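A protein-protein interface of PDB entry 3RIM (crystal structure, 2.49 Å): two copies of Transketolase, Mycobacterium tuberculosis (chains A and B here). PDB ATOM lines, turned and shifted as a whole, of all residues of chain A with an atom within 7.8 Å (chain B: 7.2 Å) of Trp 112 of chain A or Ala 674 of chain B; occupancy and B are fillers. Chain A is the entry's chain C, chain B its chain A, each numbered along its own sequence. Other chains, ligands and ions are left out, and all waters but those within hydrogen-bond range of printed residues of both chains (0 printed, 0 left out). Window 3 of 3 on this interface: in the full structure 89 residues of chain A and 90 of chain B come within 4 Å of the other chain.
No position is printed for both chains. Of the 14 pairs that touch across the chains among the printed residues, none has its exchanged pair printed and touching as well.
Printed residues of chain A that touch a printed residue of chain B: Asn 43, Arg 110, Thr 111, Trp 112, Gly 113, Pro 117 and Gly 118. Hydrophobic or aromatic side chains of chain B that line the printed part of chain A: Ala 674 and Tyr 683. Among the printed residues, 14 pairs touch across the chains. Among the printed residues, Asp or Glu carboxylates within 4 Å of a Lys or Arg side-chain nitrogen of the other chain: Arg 110 of chain A with Asp 499 of chain B.
Asn 43 of chain A touches Glu 498 of chain B. Glu 498 of chain B touches Arg 110 of chain A. Ser 673 of chain B touches Arg 110 of chain A (O to C, 3.5 Å). O of Arg 110 of chain A touches CA of Ala 674 of chain B, 3.9 Å away. CE3 of Trp 112 of chain A touches CG of Glu 672 of chain B (3.7 Å). Trp 112 of chain A touches Ser 673 of chain B. Trp 112 of chain A touches Ala 674 of chain B. CH2 of Trp 112 of chain A touches CB of Glu 682 of chain B (3.7 Å). Trp 112 of chain A touches Tyr 683 of chain B. Ser 673 of chain B touches Pro 117 of chain A (CB to CB, 3.5 Å).
The guanidinium group (NH2) of Arg 110 of chain A is in salt-bridge range of the side-chain carboxylate (OD1) of Asp 499 of chain B (3.0 Å). The side-chain carboxylate (OE2) of Glu 672 of chain B sits at hydrogen-bond distance from the backbone NH (N) of Gly 113 of chain A, 2.8 Å away. OG of Ser 673 of chain B lies within hydrogen-bond range of N of Gly 118 of chain A (3.0 Å). O of Ser 673 of chain B sits close to O of Thr 111 of chain A (3.4 Å).
The side-chain hydroxyl of Ser 673 of chain B sits at hydrogen-bond distance from the backbone carbonyl oxygen of Glu 498 of chain B, at 2.6 Å. N of Glu 498 of chain B sits at hydrogen-bond distance from O of Ala 674 of chain B (3.3 Å). OE2 of Glu 498 of chain B lies close to N of Asp 675 of chain B (3.4 Å). NE2 of Gln 504 of chain B lies within hydrogen-bond range of O of Glu 672 of chain B (2.9 Å). The side-chain amide oxygen (OD1) of Asn 43 of chain A lies within hydrogen-bond range of the guanidinium group (NE) of Arg 110 of chain A, at 2.7 Å. The backbone carbonyl oxygen of Ser 108 of chain A sits at hydrogen-bond distance from the side-chain hydroxyl of Thr 111 of chain A, at 2.7 Å.
Of the printed residues of chain B, Asn 43 of chain A touches Glu 498 (3.4 Å). Trp 112 of chain A touches five residues of chain B. Of the printed residues of chain B, Pro 117 of chain A touches Ser 673. Gly 495 of chain B touches none of the printed residues of chain A. Printed residues of chain A within 4 Å of Glu 672 of chain B: Trp 112 and Gly 113. Of chain A, only Arg 110 (3.9 Å) and Trp 112 (3.6 Å) come within 4 Å of Ala 674 of chain B. Printed residues of chain A within 4 Å of Tyr 683 of chain B: Trp 112 (3.6 Å). The nearest residue of chain B that does not touch Trp 112 of chain A is Leu 679 of chain B (4.1 Å). The nearest residue of chain A that does not touch Ala 674 of chain B is Thr 111 of chain A (4.3 Å). The nearest printed residue of chain B that does not touch Pro 117 of chain A is Glu 498 of chain B (5.3 Å).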
ATOM      1  N   VAL A  41     -25.736 -18.838 -39.740  1.00  0.00           N
ATOM      2  CA  VAL A  41     -26.354 -18.011 -38.696  1.00  0.00           C
ATOM      3  C   VAL A  41     -27.479 -17.137 -39.259  1.00  0.00           C
ATOM      4  O   VAL A  41     -28.359 -16.716 -38.502  1.00  0.00           O
ATOM      5  CB  VAL A  41     -25.285 -17.215 -37.878  1.00  0.00           C
ATOM      6  CG1 VAL A  41     -24.625 -16.190 -38.739  1.00  0.00           C
ATOM      7  CG2 VAL A  41     -25.920 -16.597 -36.638  1.00  0.00           C
ATOM      8  N   ASN A  43     -27.394 -14.069 -40.842  1.00  0.00           N
ATOM      9  CA  ASN A  43     -27.119 -12.622 -40.909  1.00  0.00           C
ATOM     10  C   ASN A  43     -25.601 -12.439 -40.892  1.00  0.00           C
ATOM     11  O   ASN A  43     -24.863 -13.353 -40.455  1.00  0.00           O
ATOM     12  CB  ASN A  43     -27.764 -11.852 -39.769  1.00  0.00           C
ATOM     13  CG  ASN A  43     -27.501 -12.479 -38.418  1.00  0.00           C
ATOM     14  OD1 ASN A  43     -26.374 -12.428 -37.891  1.00  0.00           O
ATOM     15  ND2 ASN A  43     -28.548 -13.091 -37.837  1.00  0.00           N
ATOM     16  N   SER A 108     -19.492 -20.952 -36.140  1.00  0.00           N
ATOM     17  CA  SER A 108     -20.061 -20.313 -34.973  1.00  0.00           C
ATOM     18  C   SER A 108     -20.152 -18.818 -35.181  1.00  0.00           C
ATOM     19  O   SER A 108     -20.458 -18.062 -34.232  1.00  0.00           O
ATOM     20  CB  SER A 108     -19.210 -20.601 -33.729  1.00  0.00           C
ATOM     21  OG  SER A 108     -19.111 -21.980 -33.449  1.00  0.00           O
ATOM     22  N   LEU A 109     -19.886 -18.361 -36.395  1.00  0.00           N
ATOM     23  CA  LEU A 109     -20.005 -16.937 -36.680  1.00  0.00           C
ATOM     24  C   LEU A 109     -21.226 -16.328 -35.959  1.00  0.00           C
ATOM     25  O   LEU A 109     -22.335 -16.906 -35.991  1.00  0.00           O
ATOM     26  CB  LEU A 109     -20.104 -16.709 -38.187  1.00  0.00           C
ATOM     27  CG  LEU A 109     -20.288 -15.274 -38.688  1.00  0.00           C
ATOM     28  CD1 LEU A 109     -18.922 -14.513 -38.711  1.00  0.00           C
ATOM     29  CD2 LEU A 109     -20.942 -15.237 -40.066  1.00  0.00           C
ATOM     30  N   ARG A 110     -21.007 -15.198 -35.270  1.00  0.00           N
ATOM     31  CA  ARG A 110     -22.077 -14.391 -34.645  1.00  0.00           C
ATOM     32  C   ARG A 110     -23.030 -15.133 -33.668  1.00  0.00           C
ATOM     33  O   ARG A 110     -24.212 -14.806 -33.579  1.00  0.00           O
ATOM     34  CB  ARG A 110     -22.880 -13.607 -35.709  1.00  0.00           C
ATOM     35  CG  ARG A 110     -22.021 -12.761 -36.665  1.00  0.00           C
ATOM     36  CD  ARG A 110     -22.726 -12.426 -37.981  1.00  0.00           C
ATOM     37  NE  ARG A 110     -23.864 -11.510 -37.818  1.00  0.00           N
ATOM     38  CZ  ARG A 110     -23.787 -10.178 -37.929  1.00  0.00           C
ATOM     39  NH1 ARG A 110     -22.658  -9.547 -38.118  1.00  0.00           N
ATOM     40  NH2 ARG A 110     -24.832  -9.440 -37.839  1.00  0.00           N
ATOM     41  N   THR A 111     -22.503 -16.085 -32.898  1.00  0.00           N
ATOM     42  CA  THR A 111     -23.274 -16.709 -31.805  1.00  0.00           C
ATOM     43  C   THR A 111     -22.669 -16.444 -30.417  1.00  0.00           C
ATOM     44  O   THR A 111     -21.426 -16.276 -30.278  1.00  0.00           O
ATOM     45  CB  THR A 111     -23.391 -18.250 -31.975  1.00  0.00           C
ATOM     46  OG1 THR A 111     -22.082 -18.805 -32.224  1.00  0.00           O
ATOM     47  CG2 THR A 111     -24.336 -18.602 -33.125  1.00  0.00           C
ATOM     48  N   TRP A 112     -23.541 -16.459 -29.390  1.00  0.00           N
ATOM     49  CA  TRP A 112     -23.088 -16.258 -27.999  1.00  0.00           C
ATOM     50  C   TRP A 112     -21.703 -16.911 -27.737  1.00  0.00           C
ATOM     51  O   TRP A 112     -21.560 -18.141 -27.798  1.00  0.00           O
ATOM     52  CB  TRP A 112     -24.145 -16.714 -26.992  1.00  0.00           C
ATOM     53  CG  TRP A 112     -23.738 -16.525 -25.563  1.00  0.00           C
ATOM     54  CD1 TRP A 112     -23.103 -17.449 -24.760  1.00  0.00           C
ATOM     55  CD2 TRP A 112     -23.915 -15.344 -24.740  1.00  0.00           C
ATOM     56  NE1 TRP A 112     -22.865 -16.908 -23.499  1.00  0.00           N
ATOM     57  CE2 TRP A 112     -23.358 -15.630 -23.465  1.00  0.00           C
ATOM     58  CE3 TRP A 112     -24.486 -14.088 -24.956  1.00  0.00           C
ATOM     59  CZ2 TRP A 112     -23.361 -14.706 -22.422  1.00  0.00           C
ATOM     60  CZ3 TRP A 112     -24.482 -13.163 -23.912  1.00  0.00           C
ATOM     61  CH2 TRP A 112     -23.932 -13.480 -22.661  1.00  0.00           C
ATOM     62  N   GLY A 113     -20.692 -16.053 -27.562  1.00  0.00           N
ATOM     63  CA  GLY A 113     -19.434 -16.424 -26.941  1.00  0.00           C
ATOM     64  C   GLY A 113     -18.461 -17.087 -27.870  1.00  0.00           C
ATOM     65  O   GLY A 113     -17.464 -17.635 -27.411  1.00  0.00           O
ATOM     66  N   SER A 114     -18.731 -17.040 -29.178  1.00  0.00           N
ATOM     67  CA  SER A 114     -17.881 -17.763 -30.146  1.00  0.00           C
ATOM     68  C   SER A 114     -16.592 -16.950 -30.348  1.00  0.00           C
ATOM     69  O   SER A 114     -16.518 -15.841 -29.858  1.00  0.00           O
ATOM     70  CB  SER A 114     -18.625 -17.980 -31.451  1.00  0.00           C
ATOM     71  OG  SER A 114     -18.582 -16.789 -32.181  1.00  0.00           O
ATOM     72  N   LYS A 115     -15.584 -17.516 -31.016  1.00  0.00           N
ATOM     73  CA  LYS A 115     -14.300 -16.808 -31.252  1.00  0.00           C
ATOM     74  C   LYS A 115     -14.392 -15.910 -32.484  1.00  0.00           C
ATOM     75  O   LYS A 115     -13.411 -15.245 -32.888  1.00  0.00           O
ATOM     76  CB  LYS A 115     -13.170 -17.781 -31.499  1.00  0.00           C
ATOM     77  CG  LYS A 115     -12.575 -18.378 -30.284  1.00  0.00           C
ATOM     78  CD  LYS A 115     -11.327 -19.156 -30.711  1.00  0.00           C
ATOM     79  CE  LYS A 115     -10.704 -19.880 -29.539  1.00  0.00           C
ATOM     80  NZ  LYS A 115     -11.327 -21.208 -29.364  1.00  0.00           N
ATOM     81  N   PRO A 117     -17.015 -13.217 -33.362  1.00  0.00           N
ATOM     82  CA  PRO A 117     -18.131 -12.272 -33.352  1.00  0.00           C
ATOM     83  C   PRO A 117     -18.230 -11.488 -34.681  1.00  0.00           C
ATOM     84  O   PRO A 117     -17.295 -11.459 -35.489  1.00  0.00           O
ATOM     85  CB  PRO A 117     -17.784 -11.325 -32.186  1.00  0.00           C
ATOM     86  CG  PRO A 117     -16.361 -11.320 -32.118  1.00  0.00           C
ATOM     87  CD  PRO A 117     -15.955 -12.779 -32.423  1.00  0.00           C
ATOM     88  N   GLY A 118     -19.374 -10.854 -34.870  1.00  0.00           N
ATOM     89  CA  GLY A 118     -19.619 -10.005 -36.021  1.00  0.00           C
ATOM     90  C   GLY A 118     -18.510  -9.115 -36.517  1.00  0.00           C
ATOM     91  O   GLY A 118     -18.318  -8.994 -37.751  1.00  0.00           O
ATOM     92  N   ILE B 494     -28.779  -3.441 -27.099  1.00  0.00           N
ATOM     93  CA  ILE B 494     -28.427  -4.829 -27.393  1.00  0.00           C
ATOM     94  C   ILE B 494     -29.508  -5.488 -28.303  1.00  0.00           C
ATOM     95  O   ILE B 494     -29.230  -6.428 -29.066  1.00  0.00           O
ATOM     96  CB  ILE B 494     -28.205  -5.648 -26.079  1.00  0.00           C
ATOM     97  CG1 ILE B 494     -29.370  -5.424 -25.095  1.00  0.00           C
ATOM     98  CG2 ILE B 494     -26.882  -5.257 -25.450  1.00  0.00           C
ATOM     99  CD1 ILE B 494     -29.201  -6.095 -23.790  1.00  0.00           C
ATOM    100  N   GLY B 495     -30.735  -4.976 -28.214  1.00  0.00           N
ATOM    101  CA  GLY B 495     -31.812  -5.409 -29.090  1.00  0.00           C
ATOM    102  C   GLY B 495     -31.360  -5.603 -30.527  1.00  0.00           C
ATOM    103  O   GLY B 495     -31.888  -6.469 -31.268  1.00  0.00           O
ATOM    104  N   LEU B 496     -30.371  -4.815 -30.921  1.00  0.00           N
ATOM    105  CA  LEU B 496     -29.862  -4.885 -32.275  1.00  0.00           C
ATOM    106  C   LEU B 496     -29.197  -6.237 -32.639  1.00  0.00           C
ATOM    107  O   LEU B 496     -29.004  -6.535 -33.836  1.00  0.00           O
ATOM    108  CB  LEU B 496     -28.903  -3.712 -32.500  1.00  0.00           C
ATOM    109  CG  LEU B 496     -27.404  -3.923 -32.466  1.00  0.00           C
ATOM    110  CD1 LEU B 496     -26.938  -3.889 -33.772  1.00  0.00           C
ATOM    111  CD2 LEU B 496     -26.807  -2.757 -31.934  1.00  0.00           C
ATOM    112  N   GLY B 497     -28.824  -7.021 -31.629  1.00  0.00           N
ATOM    113  CA  GLY B 497     -28.324  -8.353 -31.861  1.00  0.00           C
ATOM    114  C   GLY B 497     -26.915  -8.500 -32.395  1.00  0.00           C
ATOM    115  O   GLY B 497     -25.965  -7.888 -31.870  1.00  0.00           O
ATOM    116  N   GLU B 498     -26.781  -9.303 -33.453  1.00  0.00           N
ATOM    117  CA  GLU B 498     -25.500  -9.943 -33.796  1.00  0.00           C
ATOM    118  C   GLU B 498     -24.298  -9.064 -34.147  1.00  0.00           C
ATOM    119  O   GLU B 498     -23.154  -9.518 -34.050  1.00  0.00           O
ATOM    120  CB  GLU B 498     -25.692 -11.007 -34.887  1.00  0.00           C
ATOM    121  CG  GLU B 498     -26.400 -12.257 -34.417  1.00  0.00           C
ATOM    122  CD  GLU B 498     -27.907 -12.149 -34.520  1.00  0.00           C
ATOM    123  OE1 GLU B 498     -28.437 -11.036 -34.793  1.00  0.00           O
ATOM    124  OE2 GLU B 498     -28.586 -13.193 -34.330  1.00  0.00           O
ATOM    125  N   ASP B 499     -24.551  -7.830 -34.586  1.00  0.00           N
ATOM    126  CA  ASP B 499     -23.480  -6.871 -34.907  1.00  0.00           C
ATOM    127  C   ASP B 499     -22.534  -6.585 -33.709  1.00  0.00           C
ATOM    128  O   ASP B 499     -21.398  -6.119 -33.903  1.00  0.00           O
ATOM    129  CB  ASP B 499     -24.071  -5.573 -35.478  1.00  0.00           C
ATOM    130  CG  ASP B 499     -24.303  -5.642 -36.996  1.00  0.00           C
ATOM    131  OD1 ASP B 499     -23.876  -6.632 -37.661  1.00  0.00           O
ATOM    132  OD2 ASP B 499     -24.933  -4.699 -37.526  1.00  0.00           O
ATOM    133  N   GLY B 500     -22.966  -6.874 -32.491  1.00  0.00           N
ATOM    134  CA  GLY B 500     -22.012  -6.991 -31.412  1.00  0.00           C
ATOM    135  C   GLY B 500     -21.732  -5.717 -30.630  1.00  0.00           C
ATOM    136  O   GLY B 500     -22.408  -4.716 -30.804  1.00  0.00           O
ATOM    137  N   PRO B 501     -20.715  -5.762 -29.751  1.00  0.00           N
ATOM    138  CA  PRO B 501     -20.526  -4.715 -28.740  1.00  0.00           C
ATOM    139  C   PRO B 501     -20.005  -3.390 -29.269  1.00  0.00           C
ATOM    140  O   PRO B 501     -20.190  -2.377 -28.588  1.00  0.00           O
ATOM    141  CB  PRO B 501     -19.540  -5.345 -27.759  1.00  0.00           C
ATOM    142  CG  PRO B 501     -18.812  -6.394 -28.602  1.00  0.00           C
ATOM    143  CD  PRO B 501     -19.861  -6.941 -29.492  1.00  0.00           C
ATOM    144  N   GLN B 504     -23.568  -2.070 -30.265  1.00  0.00           N
ATOM    145  CA  GLN B 504     -24.570  -1.954 -29.227  1.00  0.00           C
ATOM    146  C   GLN B 504     -24.384  -0.758 -28.232  1.00  0.00           C
ATOM    147  O   GLN B 504     -23.351  -0.686 -27.499  1.00  0.00           O
ATOM    148  CB  GLN B 504     -24.622  -3.247 -28.469  1.00  0.00           C
ATOM    149  CG  GLN B 504     -25.124  -4.418 -29.301  1.00  0.00           C
ATOM    150  CD  GLN B 504     -24.678  -5.716 -28.711  1.00  0.00           C
ATOM    151  OE1 GLN B 504     -23.892  -5.746 -27.731  1.00  0.00           O
ATOM    152  NE2 GLN B 504     -25.171  -6.807 -29.278  1.00  0.00           N
ATOM    153  N   HIS B 669     -22.376  -3.073 -18.598  1.00  0.00           N
ATOM    154  CA  HIS B 669     -21.189  -3.505 -19.333  1.00  0.00           C
ATOM    155  C   HIS B 669     -21.513  -3.662 -20.788  1.00  0.00           C
ATOM    156  O   HIS B 669     -22.669  -3.567 -21.189  1.00  0.00           O
ATOM    157  CB  HIS B 669     -20.648  -4.821 -18.800  1.00  0.00           C
ATOM    158  CG  HIS B 669     -21.687  -5.875 -18.710  1.00  0.00           C
ATOM    159  ND1 HIS B 669     -21.769  -6.911 -19.614  1.00  0.00           N
ATOM    160  CD2 HIS B 669     -22.744  -6.021 -17.866  1.00  0.00           C
ATOM    161  CE1 HIS B 669     -22.815  -7.672 -19.317  1.00  0.00           C
ATOM    162  NE2 HIS B 669     -23.423  -7.156 -18.261  1.00  0.00           N
ATOM    163  N   GLY B 671     -21.759  -5.366 -24.620  1.00  0.00           N
ATOM    164  CA  GLY B 671     -22.573  -6.475 -25.066  1.00  0.00           C
ATOM    165  C   GLY B 671     -21.793  -7.603 -25.708  1.00  0.00           C
ATOM    166  O   GLY B 671     -20.618  -7.823 -25.402  1.00  0.00           O
ATOM    167  N   GLU B 672     -22.462  -8.313 -26.605  1.00  0.00           N
ATOM    168  CA  GLU B 672     -21.955  -9.566 -27.132  1.00  0.00           C
ATOM    169  C   GLU B 672     -22.616  -9.764 -28.477  1.00  0.00           C
ATOM    170  O   GLU B 672     -23.699  -9.198 -28.762  1.00  0.00           O
ATOM    171  CB  GLU B 672     -22.298 -10.715 -26.170  1.00  0.00           C
ATOM    172  CG  GLU B 672     -21.893 -12.109 -26.639  1.00  0.00           C
ATOM    173  CD  GLU B 672     -20.546 -12.555 -26.108  1.00  0.00           C
ATOM    174  OE1 GLU B 672     -20.082 -11.959 -25.099  1.00  0.00           O
ATOM    175  OE2 GLU B 672     -19.964 -13.506 -26.689  1.00  0.00           O
ATOM    176  N   SER B 673     -21.949 -10.550 -29.309  1.00  0.00           N
ATOM    177  CA  SER B 673     -22.425 -10.865 -30.655  1.00  0.00           C
ATOM    178  C   SER B 673     -23.325 -12.082 -30.647  1.00  0.00           C
ATOM    179  O   SER B 673     -22.820 -13.207 -30.783  1.00  0.00           O
ATOM    180  CB  SER B 673     -21.220 -11.131 -31.548  1.00  0.00           C
ATOM    181  OG  SER B 673     -21.585 -11.231 -32.899  1.00  0.00           O
ATOM    182  N   ALA B 674     -24.638 -11.868 -30.467  1.00  0.00           N
ATOM    183  CA  ALA B 674     -25.633 -12.956 -30.425  1.00  0.00           C
ATOM    184  C   ALA B 674     -27.011 -12.378 -30.742  1.00  0.00           C
ATOM    185  O   ALA B 674     -27.165 -11.162 -30.761  1.00  0.00           O
ATOM    186  CB  ALA B 674     -25.654 -13.616 -29.035  1.00  0.00           C
ATOM    187  N   ASP B 675     -28.016 -13.229 -30.961  1.00  0.00           N
ATOM    188  CA  ASP B 675     -29.370 -12.778 -31.299  1.00  0.00           C
ATOM    189  C   ASP B 675     -30.003 -12.018 -30.138  1.00  0.00           C
ATOM    190  O   ASP B 675     -29.596 -12.211 -29.016  1.00  0.00           O
ATOM    191  CB  ASP B 675     -30.240 -13.964 -31.723  1.00  0.00           C
ATOM    192  CG  ASP B 675     -30.689 -14.850 -30.547  1.00  0.00           C
ATOM    193  OD1 ASP B 675     -30.293 -14.703 -29.409  1.00  0.00           O
ATOM    194  OD2 ASP B 675     -31.482 -15.765 -30.705  1.00  0.00           O
ATOM    195  N   HIS B 676     -31.011 -11.188 -30.379  1.00  0.00           N
ATOM    196  CA  HIS B 676     -31.457 -10.299 -29.315  1.00  0.00           C
ATOM    197  C   HIS B 676     -32.076 -11.008 -28.139  1.00  0.00           C
ATOM    198  O   HIS B 676     -31.927 -10.558 -26.960  1.00  0.00           O
ATOM    199  CB  HIS B 676     -32.412  -9.230 -29.822  1.00  0.00           C
ATOM    200  CG  HIS B 676     -33.574  -9.772 -30.593  1.00  0.00           C
ATOM    201  ND1 HIS B 676     -34.845  -9.836 -30.088  1.00  0.00           N
ATOM    202  CD2 HIS B 676     -33.666 -10.236 -31.850  1.00  0.00           C
ATOM    203  CE1 HIS B 676     -35.666 -10.327 -30.995  1.00  0.00           C
ATOM    204  NE2 HIS B 676     -34.972 -10.587 -32.074  1.00  0.00           N
ATOM    205  N   LYS B 677     -32.799 -12.095 -28.444  1.00  0.00           N
ATOM    206  CA  LYS B 677     -33.522 -12.806 -27.379  1.00  0.00           C
ATOM    207  C   LYS B 677     -32.548 -13.415 -26.380  1.00  0.00           C
ATOM    208  O   LYS B 677     -32.764 -13.305 -25.169  1.00  0.00           O
ATOM    209  CB  LYS B 677     -34.509 -13.844 -27.914  1.00  0.00           C
ATOM    210  CG  LYS B 677     -35.886 -13.225 -28.181  1.00  0.00           C
ATOM    211  CD  LYS B 677     -37.028 -14.264 -28.223  1.00  0.00           C
ATOM    212  CE  LYS B 677     -37.522 -14.526 -29.664  1.00  0.00           C
ATOM    213  NZ  LYS B 677     -36.394 -14.897 -30.592  1.00  0.00           N
ATOM    214  N   THR B 678     -31.478 -14.011 -26.891  1.00  0.00           N
ATOM    215  CA  THR B 678     -30.393 -14.495 -26.045  1.00  0.00           C
ATOM    216  C   THR B 678     -29.800 -13.359 -25.206  1.00  0.00           C
ATOM    217  O   THR B 678     -29.545 -13.531 -24.026  1.00  0.00           O
ATOM    218  CB  THR B 678     -29.274 -15.184 -26.885  1.00  0.00           C
ATOM    219  OG1 THR B 678     -29.852 -16.167 -27.747  1.00  0.00           O
ATOM    220  CG2 THR B 678     -28.249 -15.872 -25.999  1.00  0.00           C
ATOM    221  N   LEU B 679     -29.619 -12.197 -25.814  1.00  0.00           N
ATOM    222  CA  LEU B 679     -28.982 -11.069 -25.142  1.00  0.00           C
ATOM    223  C   LEU B 679     -29.808 -10.522 -24.003  1.00  0.00           C
ATOM    224  O   LEU B 679     -29.311 -10.372 -22.876  1.00  0.00           O
ATOM    225  CB  LEU B 679     -28.598  -9.950 -26.128  1.00  0.00           C
ATOM    226  CG  LEU B 679     -27.456 -10.147 -27.144  1.00  0.00           C
ATOM    227  CD1 LEU B 679     -27.351  -8.867 -27.928  1.00  0.00           C
ATOM    228  CD2 LEU B 679     -26.135 -10.453 -26.533  1.00  0.00           C
ATOM    229  N   GLU B 682     -29.831 -13.262 -21.172  1.00  0.00           N
ATOM    230  CA  GLU B 682     -28.549 -13.316 -20.466  1.00  0.00           C
ATOM    231  C   GLU B 682     -28.270 -12.110 -19.581  1.00  0.00           C
ATOM    232  O   GLU B 682     -27.634 -12.259 -18.566  1.00  0.00           O
ATOM    233  CB  GLU B 682     -27.385 -13.506 -21.439  1.00  0.00           C
ATOM    234  CG  GLU B 682     -27.362 -14.867 -22.170  1.00  0.00           C
ATOM    235  CD  GLU B 682     -27.219 -16.083 -21.255  1.00  0.00           C
ATOM    236  OE1 GLU B 682     -27.030 -15.917 -20.019  1.00  0.00           O
ATOM    237  OE2 GLU B 682     -27.299 -17.217 -21.786  1.00  0.00           O
ATOM    238  N   TYR B 683     -28.742 -10.926 -19.961  1.00  0.00           N
ATOM    239  CA  TYR B 683     -28.417  -9.707 -19.213  1.00  0.00           C
ATOM    240  C   TYR B 683     -29.539  -9.329 -18.282  1.00  0.00           C
ATOM    241  O   TYR B 683     -29.542  -8.253 -17.679  1.00  0.00           O
ATOM    242  CB  TYR B 683     -28.042  -8.575 -20.171  1.00  0.00           C
ATOM    243  CG  TYR B 683     -26.793  -8.902 -20.977  1.00  0.00           C
ATOM    244  CD1 TYR B 683     -25.767  -9.690 -20.423  1.00  0.00           C
ATOM    245  CD2 TYR B 683     -26.623  -8.424 -22.277  1.00  0.00           C
ATOM    246  CE1 TYR B 683     -24.619 -10.007 -21.163  1.00  0.00           C
ATOM    247  CE2 TYR B 683     -25.475  -8.721 -23.011  1.00  0.00           C
ATOM    248  CZ  TYR B 683     -24.486  -9.514 -22.455  1.00  0.00           C
ATOM    249  OH  TYR B 683     -23.341  -9.817 -23.160  1.00  0.00           O
